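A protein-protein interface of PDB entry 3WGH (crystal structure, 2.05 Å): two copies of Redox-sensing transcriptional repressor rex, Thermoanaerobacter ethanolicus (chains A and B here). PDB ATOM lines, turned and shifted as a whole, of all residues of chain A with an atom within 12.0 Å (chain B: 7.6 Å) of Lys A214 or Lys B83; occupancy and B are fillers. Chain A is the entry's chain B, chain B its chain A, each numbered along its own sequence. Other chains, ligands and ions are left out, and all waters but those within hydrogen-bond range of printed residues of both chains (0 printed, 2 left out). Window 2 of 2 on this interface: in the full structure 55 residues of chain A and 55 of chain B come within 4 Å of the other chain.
O of Leu B79 is in hydrogen-bond range of OG of Ser A203.
The backbone carbonyl oxygen (O) of Leu B79 sits at hydrogen-bond distance from the backbone NH (N) of Tyr A204 (3.2 Å).
The side-chain amino group (NZ) of Lys B83 lies within hydrogen-bond range of the side-chain amide oxygen (OD1) of Asn A207, at 3.1 Å.
The side-chain amide nitrogen (ND2) of Asn A207 sits close to the side-chain hydroxyl (OH) of Tyr B85 (2.4 Å).
CE2 of Phe B110 touches CG of Leu A199, at 3.9 Å.
Leu B79 touches Phe A200.
Phe A200 touches Leu B81.
Ser B108 touches Phe A200 (OG to CZ, 3.7 Å).
OG of Ser A203 touches CD2 of Leu B81 (3.7 Å).
Ser A203 touches Tyr B85.
Ser A203 touches Phe B110 (CB to CZ, 3.8 Å).
CE1 of Tyr B85 touches CD1 of Leu A206, at 3.8 Å.
Asn A207 touches Gly B80 (ND2 to CA, 3.6 Å).
Leu A211 touches Lys B77.
Of chain B, only Lys B83 (3.8 Å) comes within 4 Å of Lys A214.
Lys B83 touches just these residues of chain A: Asn A207 (3.1 Å) and Lys A214 (3.8 Å).
Of chain A, only Phe A200 and Ser A203 come within 4 Å of Leu B81.
No residue of chain A comes within 4 Å of Asp B82.
Of the printed residues of chain B, Tyr A204 touches Leu B79 (3.2 Å).
Printed residues of chain B within 4 Å of Phe A200: Leu B79 (3.8 Å), Leu B81 (3.8 Å), Ser B108 (3.7 Å) and Phe B110 (3.8 Å).
Of the printed residues of chain B, Asn A207 touches Gly B80 (3.6 Å), Lys B83 (3.1 Å) and Tyr B85 (2.4 Å).
Of the printed residues of chain A, Leu B79 touches Phe A200, Ser A203 and Tyr A204.
Of the printed residues of chain B, Leu A211 touches Lys B77.
Lys A216 touches none of the printed residues of chain B.
Asn B111 touches none of the printed residues of chain A.
The nearest residue of chain B that does not touch Lys A214 is Lys B77 (4.8 Å).
Hydrophobic or aromatic side chains of chain B that line the printed part of chain A: Leu B79, Leu B81, Tyr B85 and Phe B110.
Along chain B the printed residues that touch a printed residue of chain A span positions 77 to 110.
Of the 17 printed residues of chain A, 8 touch a printed residue of chain B.
Hydrophobic or aromatic side chains of chain A that line the printed part of chain B: Leu A199, Phe A200, Leu A206 and Leu A211.
Among the printed residues, no Asp or Glu carboxylate lies within 4 Å of a Lys or Arg side-chain nitrogen of the other chain.
No position is printed for both chains.
The backbone carbonyl oxygen (O) of Thr B76 sits at hydrogen-bond distance from the backbone NH (N) of Leu B81, at 2.8 Å.
The backbone carbonyl oxygen (O) of Gly B80 is in hydrogen-bond range of the side-chain hydroxyl (OH) of Tyr B85 (2.7 Å).
The backbone carbonyl oxygen (O) of Gly B109 is in hydrogen-bond range of the backbone NH (N) of Tyr B85 (2.5 Å).
N of Asn B111 lies within hydrogen-bond range of O of Tyr B85 (2.8 Å).
O of Phe A200 sits at hydrogen-bond distance from OG of Ser A203, at 2.9 Å.
The side-chain amide nitrogen (ND2) of Asn A207 sits at hydrogen-bond distance from the backbone carbonyl oxygen (O) of Ser A203.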
ATOM      1  N   LEU A 199      21.032 -27.734  10.641  1.00  0.00           N
ATOM      2  CA  LEU A 199      21.257 -26.328  10.304  1.00  0.00           C
ATOM      3  C   LEU A 199      19.999 -25.452  10.428  1.00  0.00           C
ATOM      4  O   LEU A 199      20.057 -24.268  10.898  1.00  0.00           O
ATOM      5  CB  LEU A 199      21.829 -26.215   8.884  1.00  0.00           C
ATOM      6  CG  LEU A 199      22.153 -24.751   8.521  1.00  0.00           C
ATOM      7  CD1 LEU A 199      23.226 -24.144   9.485  1.00  0.00           C
ATOM      8  CD2 LEU A 199      22.669 -24.740   7.126  1.00  0.00           C
ATOM      9  N   PHE A 200      18.878 -25.996   9.988  1.00  0.00           N
ATOM     10  CA  PHE A 200      17.630 -25.245  10.039  1.00  0.00           C
ATOM     11  C   PHE A 200      17.087 -25.011  11.456  1.00  0.00           C
ATOM     12  O   PHE A 200      16.196 -24.146  11.665  1.00  0.00           O
ATOM     13  CB  PHE A 200      16.548 -25.926   9.182  1.00  0.00           C
ATOM     14  CG  PHE A 200      16.835 -25.912   7.713  1.00  0.00           C
ATOM     15  CD1 PHE A 200      17.961 -25.283   7.211  1.00  0.00           C
ATOM     16  CD2 PHE A 200      15.987 -26.575   6.832  1.00  0.00           C
ATOM     17  CE1 PHE A 200      18.230 -25.297   5.841  1.00  0.00           C
ATOM     18  CE2 PHE A 200      16.241 -26.562   5.430  1.00  0.00           C
ATOM     19  CZ  PHE A 200      17.330 -25.910   4.951  1.00  0.00           C
ATOM     20  N   VAL A 202      19.073 -23.855  13.610  1.00  0.00           N
ATOM     21  CA  VAL A 202      19.840 -22.629  14.004  1.00  0.00           C
ATOM     22  C   VAL A 202      19.118 -21.390  13.487  1.00  0.00           C
ATOM     23  O   VAL A 202      18.844 -20.447  14.235  1.00  0.00           O
ATOM     24  CB  VAL A 202      21.271 -22.700  13.496  1.00  0.00           C
ATOM     25  CG1 VAL A 202      22.030 -21.317  13.695  1.00  0.00           C
ATOM     26  CG2 VAL A 202      22.012 -23.888  14.142  1.00  0.00           C
ATOM     27  N   SER A 203      18.734 -21.427  12.203  1.00  0.00           N
ATOM     28  CA  SER A 203      17.834 -20.393  11.695  1.00  0.00           C
ATOM     29  C   SER A 203      16.517 -20.253  12.475  1.00  0.00           C
ATOM     30  O   SER A 203      16.095 -19.135  12.748  1.00  0.00           O
ATOM     31  CB  SER A 203      17.554 -20.602  10.236  1.00  0.00           C
ATOM     32  OG  SER A 203      17.024 -21.895  10.031  1.00  0.00           O
ATOM     33  N   TYR A 204      15.936 -21.362  12.930  1.00  0.00           N
ATOM     34  CA  TYR A 204      14.724 -21.284  13.754  1.00  0.00           C
ATOM     35  C   TYR A 204      14.979 -20.469  14.995  1.00  0.00           C
ATOM     36  O   TYR A 204      14.259 -19.541  15.278  1.00  0.00           O
ATOM     37  CB  TYR A 204      14.223 -22.663  14.159  1.00  0.00           C
ATOM     38  CG  TYR A 204      13.062 -22.562  15.098  1.00  0.00           C
ATOM     39  CD1 TYR A 204      13.287 -22.499  16.476  1.00  0.00           C
ATOM     40  CD2 TYR A 204      11.747 -22.496  14.633  1.00  0.00           C
ATOM     41  CE1 TYR A 204      12.275 -22.366  17.372  1.00  0.00           C
ATOM     42  CE2 TYR A 204      10.673 -22.343  15.549  1.00  0.00           C
ATOM     43  CZ  TYR A 204      10.971 -22.278  16.929  1.00  0.00           C
ATOM     44  OH  TYR A 204      10.001 -22.171  17.915  1.00  0.00           O
ATOM     45  N   ARG A 205      16.028 -20.837  15.720  1.00  0.00           N
ATOM     46  CA  ARG A 205      16.356 -20.218  17.002  1.00  0.00           C
ATOM     47  C   ARG A 205      16.824 -18.787  16.872  1.00  0.00           C
ATOM     48  O   ARG A 205      16.505 -17.977  17.737  1.00  0.00           O
ATOM     49  CB  ARG A 205      17.406 -21.049  17.737  1.00  0.00           C
ATOM     50  CG  ARG A 205      16.844 -22.270  18.430  1.00  0.00           C
ATOM     51  CD  ARG A 205      17.989 -23.050  19.100  1.00  0.00           C
ATOM     52  NE  ARG A 205      18.556 -23.996  18.144  1.00  0.00           N
ATOM     53  CZ  ARG A 205      19.427 -24.957  18.479  1.00  0.00           C
ATOM     54  NH1 ARG A 205      19.846 -25.061  19.748  1.00  0.00           N
ATOM     55  NH2 ARG A 205      19.893 -25.809  17.559  1.00  0.00           N
ATOM     56  N   LEU A 206      17.594 -18.469  15.827  1.00  0.00           N
ATOM     57  CA  LEU A 206      17.842 -17.067  15.505  1.00  0.00           C
ATOM     58  C   LEU A 206      16.555 -16.197  15.404  1.00  0.00           C
ATOM     59  O   LEU A 206      16.534 -15.057  15.876  1.00  0.00           O
ATOM     60  CB  LEU A 206      18.721 -16.944  14.259  1.00  0.00           C
ATOM     61  CG  LEU A 206      20.205 -17.276  14.521  1.00  0.00           C
ATOM     62  CD1 LEU A 206      20.984 -17.434  13.234  1.00  0.00           C
ATOM     63  CD2 LEU A 206      20.920 -16.248  15.501  1.00  0.00           C
ATOM     64  N   ASN A 207      15.460 -16.741  14.873  1.00  0.00           N
ATOM     65  CA  ASN A 207      14.255 -15.944  14.614  1.00  0.00           C
ATOM     66  C   ASN A 207      13.066 -16.187  15.512  1.00  0.00           C
ATOM     67  O   ASN A 207      11.975 -15.696  15.198  1.00  0.00           O
ATOM     68  CB  ASN A 207      13.731 -16.279  13.227  1.00  0.00           C
ATOM     69  CG  ASN A 207      14.507 -15.620  12.155  1.00  0.00           C
ATOM     70  OD1 ASN A 207      14.262 -14.452  11.803  1.00  0.00           O
ATOM     71  ND2 ASN A 207      15.453 -16.358  11.598  1.00  0.00           N
ATOM     72  N   GLU A 208      13.211 -17.052  16.503  1.00  0.00           N
ATOM     73  CA  GLU A 208      12.090 -17.482  17.296  1.00  0.00           C
ATOM     74  C   GLU A 208      11.455 -16.325  18.084  1.00  0.00           C
ATOM     75  O   GLU A 208      10.213 -16.172  18.100  1.00  0.00           O
ATOM     76  CB  GLU A 208      12.484 -18.590  18.275  1.00  0.00           C
ATOM     77  CG  GLU A 208      11.243 -19.324  18.768  1.00  0.00           C
ATOM     78  CD  GLU A 208      11.480 -20.222  19.947  1.00  0.00           C
ATOM     79  OE1 GLU A 208      10.852 -21.320  19.996  1.00  0.00           O
ATOM     80  OE2 GLU A 208      12.296 -19.846  20.816  1.00  0.00           O
ATOM     81  N   GLU A 209      12.298 -15.525  18.743  1.00  0.00           N
ATOM     82  CA  GLU A 209      11.810 -14.348  19.482  1.00  0.00           C
ATOM     83  C   GLU A 209      10.909 -13.491  18.584  1.00  0.00           C
ATOM     84  O   GLU A 209       9.738 -13.321  18.912  1.00  0.00           O
ATOM     85  CB  GLU A 209      12.962 -13.540  20.080  1.00  0.00           C
ATOM     86  CG  GLU A 209      12.513 -12.498  21.091  1.00  0.00           C
ATOM     87  CD  GLU A 209      13.692 -11.887  21.888  1.00  0.00           C
ATOM     88  OE1 GLU A 209      14.325 -12.603  22.702  1.00  0.00           O
ATOM     89  OE2 GLU A 209      13.974 -10.688  21.692  1.00  0.00           O
ATOM     90  N   GLU A 210      11.429 -12.989  17.458  1.00  0.00           N
ATOM     91  CA  GLU A 210      10.593 -12.247  16.484  1.00  0.00           C
ATOM     92  C   GLU A 210       9.308 -13.015  16.174  1.00  0.00           C
ATOM     93  O   GLU A 210       8.189 -12.538  16.439  1.00  0.00           O
ATOM     94  CB  GLU A 210      11.313 -11.967  15.146  1.00  0.00           C
ATOM     95  CG  GLU A 210      12.424 -10.882  15.162  1.00  0.00           C
ATOM     96  CD  GLU A 210      11.933  -9.438  15.465  1.00  0.00           C
ATOM     97  OE1 GLU A 210      12.428  -8.491  14.797  1.00  0.00           O
ATOM     98  OE2 GLU A 210      11.073  -9.242  16.369  1.00  0.00           O
ATOM     99  N   LEU A 211       9.484 -14.214  15.624  1.00  0.00           N
ATOM    100  CA  LEU A 211       8.360 -15.008  15.157  1.00  0.00           C
ATOM    101  C   LEU A 211       7.192 -14.811  16.109  1.00  0.00           C
ATOM    102  O   LEU A 211       6.080 -14.513  15.673  1.00  0.00           O
ATOM    103  CB  LEU A 211       8.728 -16.507  15.097  1.00  0.00           C
ATOM    104  CG  LEU A 211       7.616 -17.469  14.670  1.00  0.00           C
ATOM    105  CD1 LEU A 211       7.222 -17.159  13.234  1.00  0.00           C
ATOM    106  CD2 LEU A 211       8.056 -18.977  14.815  1.00  0.00           C
ATOM    107  N   PHE A 212       7.463 -15.002  17.400  1.00  0.00           N
ATOM    108  CA  PHE A 212       6.443 -14.876  18.439  1.00  0.00           C
ATOM    109  C   PHE A 212       5.939 -13.466  18.722  1.00  0.00           C
ATOM    110  O   PHE A 212       4.735 -13.275  18.808  1.00  0.00           O
ATOM    111  CB  PHE A 212       6.811 -15.650  19.696  1.00  0.00           C
ATOM    112  CG  PHE A 212       6.603 -17.086  19.517  1.00  0.00           C
ATOM    113  CD1 PHE A 212       5.360 -17.639  19.765  1.00  0.00           C
ATOM    114  CD2 PHE A 212       7.578 -17.857  18.890  1.00  0.00           C
ATOM    115  CE1 PHE A 212       5.117 -18.979  19.506  1.00  0.00           C
ATOM    116  CE2 PHE A 212       7.365 -19.203  18.613  1.00  0.00           C
ATOM    117  CZ  PHE A 212       6.140 -19.773  18.922  1.00  0.00           C
ATOM    118  N   LYS A 213       6.834 -12.485  18.787  1.00  0.00           N
ATOM    119  CA  LYS A 213       6.412 -11.079  18.735  1.00  0.00           C
ATOM    120  C   LYS A 213       5.272 -10.982  17.712  1.00  0.00           C
ATOM    121  O   LYS A 213       4.197 -10.472  18.035  1.00  0.00           O
ATOM    122  CB  LYS A 213       7.564 -10.150  18.304  1.00  0.00           C
ATOM    123  CG  LYS A 213       8.472  -9.601  19.418  1.00  0.00           C
ATOM    124  CD  LYS A 213       9.192  -8.318  18.928  1.00  0.00           C
ATOM    125  CE  LYS A 213      10.256  -7.792  19.907  1.00  0.00           C
ATOM    126  NZ  LYS A 213      10.505  -6.312  19.745  1.00  0.00           N
ATOM    127  N   LYS A 214       5.491 -11.512  16.500  1.00  0.00           N
ATOM    128  CA  LYS A 214       4.503 -11.380  15.412  1.00  0.00           C
ATOM    129  C   LYS A 214       3.164 -12.046  15.717  1.00  0.00           C
ATOM    130  O   LYS A 214       2.097 -11.427  15.563  1.00  0.00           O
ATOM    131  CB  LYS A 214       5.053 -11.873  14.068  1.00  0.00           C
ATOM    132  CG  LYS A 214       5.937 -10.844  13.365  1.00  0.00           C
ATOM    133  CD  LYS A 214       6.707 -11.473  12.209  1.00  0.00           C
ATOM    134  CE  LYS A 214       7.895 -10.618  11.784  1.00  0.00           C
ATOM    135  NZ  LYS A 214       8.716 -11.359  10.765  1.00  0.00           N
ATOM    136  N   LEU A 215       3.225 -13.296  16.160  1.00  0.00           N
ATOM    137  CA  LEU A 215       2.017 -14.067  16.388  1.00  0.00           C
ATOM    138  C   LEU A 215       1.112 -13.437  17.459  1.00  0.00           C
ATOM    139  O   LEU A 215      -0.111 -13.430  17.307  1.00  0.00           O
ATOM    140  CB  LEU A 215       2.363 -15.519  16.719  1.00  0.00           C
ATOM    141  CG  LEU A 215       3.504 -16.151  15.908  1.00  0.00           C
ATOM    142  CD1 LEU A 215       3.750 -17.600  16.335  1.00  0.00           C
ATOM    143  CD2 LEU A 215       3.312 -16.033  14.376  1.00  0.00           C
ATOM    144  N   LYS A 216       1.709 -12.866  18.508  1.00  0.00           N
ATOM    145  CA  LYS A 216       0.937 -12.157  19.543  1.00  0.00           C
ATOM    146  C   LYS A 216       0.613 -10.693  19.191  1.00  0.00           C
ATOM    147  O   LYS A 216      -0.192 -10.409  18.298  1.00  0.00           O
ATOM    148  CB  LYS A 216       1.638 -12.248  20.912  1.00  0.00           C
ATOM    149  CG  LYS A 216       1.605 -13.656  21.547  1.00  0.00           C
ATOM    150  CD  LYS A 216       2.904 -14.453  21.299  1.00  0.00           C
ATOM    151  CE  LYS A 216       2.751 -15.931  21.703  1.00  0.00           C
ATOM    152  NZ  LYS A 216       3.882 -16.446  22.577  1.00  0.00           N
ATOM    153  N   THR B  76       8.467 -22.588   5.960  1.00  0.00           N
ATOM    154  CA  THR B  76       9.636 -21.765   5.575  1.00  0.00           C
ATOM    155  C   THR B  76       9.791 -20.556   6.507  1.00  0.00           C
ATOM    156  O   THR B  76      10.896 -20.237   6.957  1.00  0.00           O
ATOM    157  CB  THR B  76       9.515 -21.305   4.071  1.00  0.00           C
ATOM    158  OG1 THR B  76       9.515 -22.453   3.219  1.00  0.00           O
ATOM    159  CG2 THR B  76      10.640 -20.343   3.647  1.00  0.00           C
ATOM    160  N   LYS B  77       8.672 -19.895   6.797  1.00  0.00           N
ATOM    161  CA  LYS B  77       8.649 -18.736   7.681  1.00  0.00           C
ATOM    162  C   LYS B  77       8.967 -19.097   9.138  1.00  0.00           C
ATOM    163  O   LYS B  77       9.773 -18.419   9.777  1.00  0.00           O
ATOM    164  CB  LYS B  77       7.283 -18.045   7.559  1.00  0.00           C
ATOM    165  CG  LYS B  77       7.048 -16.940   8.582  1.00  0.00           C
ATOM    166  CD  LYS B  77       5.520 -16.693   8.720  1.00  0.00           C
ATOM    167  CE  LYS B  77       5.120 -16.518  10.191  1.00  0.00           C
ATOM    168  NZ  LYS B  77       4.349 -15.248  10.478  1.00  0.00           N
ATOM    169  N   LEU B  79      10.707 -21.666  10.268  1.00  0.00           N
ATOM    170  CA  LEU B  79      12.118 -21.976  10.322  1.00  0.00           C
ATOM    171  C   LEU B  79      13.079 -20.830  10.082  1.00  0.00           C
ATOM    172  O   LEU B  79      14.306 -21.016  10.178  1.00  0.00           O
ATOM    173  CB  LEU B  79      12.422 -23.073   9.327  1.00  0.00           C
ATOM    174  CG  LEU B  79      11.781 -24.372   9.744  1.00  0.00           C
ATOM    175  CD1 LEU B  79      11.878 -25.345   8.584  1.00  0.00           C
ATOM    176  CD2 LEU B  79      12.513 -24.889  10.977  1.00  0.00           C
ATOM    177  N   GLY B  80      12.545 -19.642   9.798  1.00  0.00           N
ATOM    178  CA  GLY B  80      13.388 -18.510   9.541  1.00  0.00           C
ATOM    179  C   GLY B  80      14.047 -18.577   8.177  1.00  0.00           C
ATOM    180  O   GLY B  80      15.061 -17.888   7.939  1.00  0.00           O
ATOM    181  N   LEU B  81      13.497 -19.382   7.280  1.00  0.00           N
ATOM    182  CA  LEU B  81      14.138 -19.583   5.973  1.00  0.00           C
ATOM    183  C   LEU B  81      13.744 -18.549   4.915  1.00  0.00           C
ATOM    184  O   LEU B  81      14.131 -18.674   3.744  1.00  0.00           O
ATOM    185  CB  LEU B  81      13.899 -20.982   5.433  1.00  0.00           C
ATOM    186  CG  LEU B  81      14.517 -22.096   6.290  1.00  0.00           C
ATOM    187  CD1 LEU B  81      14.184 -23.433   5.650  1.00  0.00           C
ATOM    188  CD2 LEU B  81      16.045 -21.879   6.424  1.00  0.00           C
ATOM    189  N   ASP B  82      12.992 -17.530   5.319  1.00  0.00           N
ATOM    190  CA  ASP B  82      12.736 -16.409   4.430  1.00  0.00           C
ATOM    191  C   ASP B  82      13.746 -15.317   4.595  1.00  0.00           C
ATOM    192  O   ASP B  82      13.628 -14.281   3.932  1.00  0.00           O
ATOM    193  CB  ASP B  82      11.334 -15.804   4.633  1.00  0.00           C
ATOM    194  CG  ASP B  82      10.942 -15.691   6.090  1.00  0.00           C
ATOM    195  OD1 ASP B  82      11.801 -15.818   7.021  1.00  0.00           O
ATOM    196  OD2 ASP B  82       9.710 -15.552   6.306  1.00  0.00           O
ATOM    197  N   LYS B  83      14.698 -15.520   5.511  1.00  0.00           N
ATOM    198  CA  LYS B  83      15.751 -14.563   5.791  1.00  0.00           C
ATOM    199  C   LYS B  83      17.075 -15.070   5.257  1.00  0.00           C
ATOM    200  O   LYS B  83      17.164 -16.143   4.670  1.00  0.00           O
ATOM    201  CB  LYS B  83      15.797 -14.200   7.286  1.00  0.00           C
ATOM    202  CG  LYS B  83      14.732 -13.101   7.594  1.00  0.00           C
ATOM    203  CD  LYS B  83      14.326 -13.019   9.065  1.00  0.00           C
ATOM    204  CE  LYS B  83      12.991 -12.303   9.247  1.00  0.00           C
ATOM    205  NZ  LYS B  83      12.083 -13.014  10.219  1.00  0.00           N
ATOM    206  N   THR B  84      18.101 -14.269   5.394  1.00  0.00           N
ATOM    207  CA  THR B  84      19.355 -14.563   4.732  1.00  0.00           C
ATOM    208  C   THR B  84      20.343 -14.533   5.893  1.00  0.00           C
ATOM    209  O   THR B  84      20.188 -13.690   6.798  1.00  0.00           O
ATOM    210  CB  THR B  84      19.635 -13.431   3.668  1.00  0.00           C
ATOM    211  OG1 THR B  84      20.762 -13.766   2.863  1.00  0.00           O
ATOM    212  CG2 THR B  84      19.902 -12.122   4.350  1.00  0.00           C
ATOM    213  N   TYR B  85      21.286 -15.484   5.934  1.00  0.00           N
ATOM    214  CA  TYR B  85      22.282 -15.510   7.028  1.00  0.00           C
ATOM    215  C   TYR B  85      23.663 -15.519   6.448  1.00  0.00           C
ATOM    216  O   TYR B  85      23.931 -16.292   5.520  1.00  0.00           O
ATOM    217  CB  TYR B  85      22.154 -16.748   7.927  1.00  0.00           C
ATOM    218  CG  TYR B  85      20.769 -16.902   8.441  1.00  0.00           C
ATOM    219  CD1 TYR B  85      20.412 -16.348   9.665  1.00  0.00           C
ATOM    220  CD2 TYR B  85      19.793 -17.580   7.680  1.00  0.00           C
ATOM    221  CE1 TYR B  85      19.112 -16.423  10.125  1.00  0.00           C
ATOM    222  CE2 TYR B  85      18.462 -17.659   8.143  1.00  0.00           C
ATOM    223  CZ  TYR B  85      18.157 -17.070   9.376  1.00  0.00           C
ATOM    224  OH  TYR B  85      16.869 -17.095   9.828  1.00  0.00           O
ATOM    225  N   GLU B 106      23.222 -22.451   0.537  1.00  0.00           N
ATOM    226  CA  GLU B 106      23.184 -21.184  -0.184  1.00  0.00           C
ATOM    227  C   GLU B 106      21.785 -20.860  -0.663  1.00  0.00           C
ATOM    228  O   GLU B 106      21.236 -19.795  -0.351  1.00  0.00           O
ATOM    229  CB  GLU B 106      24.142 -21.225  -1.385  1.00  0.00           C
ATOM    230  CG  GLU B 106      25.614 -21.136  -1.024  1.00  0.00           C
ATOM    231  CD  GLU B 106      26.190 -19.738  -1.252  1.00  0.00           C
ATOM    232  OE1 GLU B 106      25.924 -19.144  -2.329  1.00  0.00           O
ATOM    233  OE2 GLU B 106      26.919 -19.247  -0.358  1.00  0.00           O
ATOM    234  N   LYS B 107      21.198 -21.797  -1.401  1.00  0.00           N
ATOM    235  CA  LYS B 107      19.853 -21.625  -1.916  1.00  0.00           C
ATOM    236  C   LYS B 107      18.838 -21.424  -0.796  1.00  0.00           C
ATOM    237  O   LYS B 107      17.799 -20.820  -1.013  1.00  0.00           O
ATOM    238  CB  LYS B 107      19.459 -22.789  -2.851  1.00  0.00           C
ATOM    239  CG  LYS B 107      19.910 -22.591  -4.310  1.00  0.00           C
ATOM    240  CD  LYS B 107      21.445 -22.456  -4.414  1.00  0.00           C
ATOM    241  CE  LYS B 107      21.871 -21.315  -5.344  1.00  0.00           C
ATOM    242  NZ  LYS B 107      23.256 -20.822  -4.995  1.00  0.00           N
ATOM    243  N   SER B 108      19.164 -21.875   0.420  1.00  0.00           N
ATOM    244  CA  SER B 108      18.256 -21.709   1.561  1.00  0.00           C
ATOM    245  C   SER B 108      18.468 -20.435   2.395  1.00  0.00           C
ATOM    246  O   SER B 108      17.786 -20.241   3.402  1.00  0.00           O
ATOM    247  CB  SER B 108      18.300 -22.947   2.453  1.00  0.00           C
ATOM    248  OG  SER B 108      17.789 -24.056   1.758  1.00  0.00           O
ATOM    249  N   GLY B 109      19.378 -19.558   1.981  1.00  0.00           N
ATOM    250  CA  GLY B 109      19.594 -18.328   2.727  1.00  0.00           C
ATOM    251  C   GLY B 109      20.881 -18.297   3.520  1.00  0.00           C
ATOM    252  O   GLY B 109      21.138 -17.328   4.234  1.00  0.00           O
ATOM    253  N   PHE B 110      21.725 -19.317   3.357  1.00  0.00           N
ATOM    254  CA  PHE B 110      23.005 -19.394   4.091  1.00  0.00           C
ATOM    255  C   PHE B 110      24.164 -19.032   3.186  1.00  0.00           C
ATOM    256  O   PHE B 110      24.798 -19.880   2.555  1.00  0.00           O
ATOM    257  CB  PHE B 110      23.191 -20.775   4.722  1.00  0.00           C
ATOM    258  CG  PHE B 110      22.099 -21.114   5.696  1.00  0.00           C
ATOM    259  CD1 PHE B 110      20.918 -21.682   5.244  1.00  0.00           C
ATOM    260  CD2 PHE B 110      22.224 -20.769   7.045  1.00  0.00           C
ATOM    261  CE1 PHE B 110      19.842 -21.912   6.131  1.00  0.00           C
ATOM    262  CE2 PHE B 110      21.186 -21.030   7.936  1.00  0.00           C
ATOM    263  CZ  PHE B 110      19.988 -21.613   7.483  1.00  0.00           C
ATOM    264  N   ASN B 111      24.414 -17.736   3.112  1.00  0.00           N
ATOM    265  CA  ASN B 111      25.412 -17.252   2.192  1.00  0.00           C
ATOM    266  C   ASN B 111      26.763 -17.316   2.867  1.00  0.00           C
ATOM    267  O   ASN B 111      26.960 -16.714   3.889  1.00  0.00           O
ATOM    268  CB  ASN B 111      25.080 -15.840   1.702  1.00  0.00           C
ATOM    269  CG  ASN B 111      23.714 -15.768   0.991  1.00  0.00           C
ATOM    270  OD1 ASN B 111      22.949 -14.828   1.236  1.00  0.00           O
ATOM    271  ND2 ASN B 111      23.401 -16.752   0.121  1.00  0.00           N
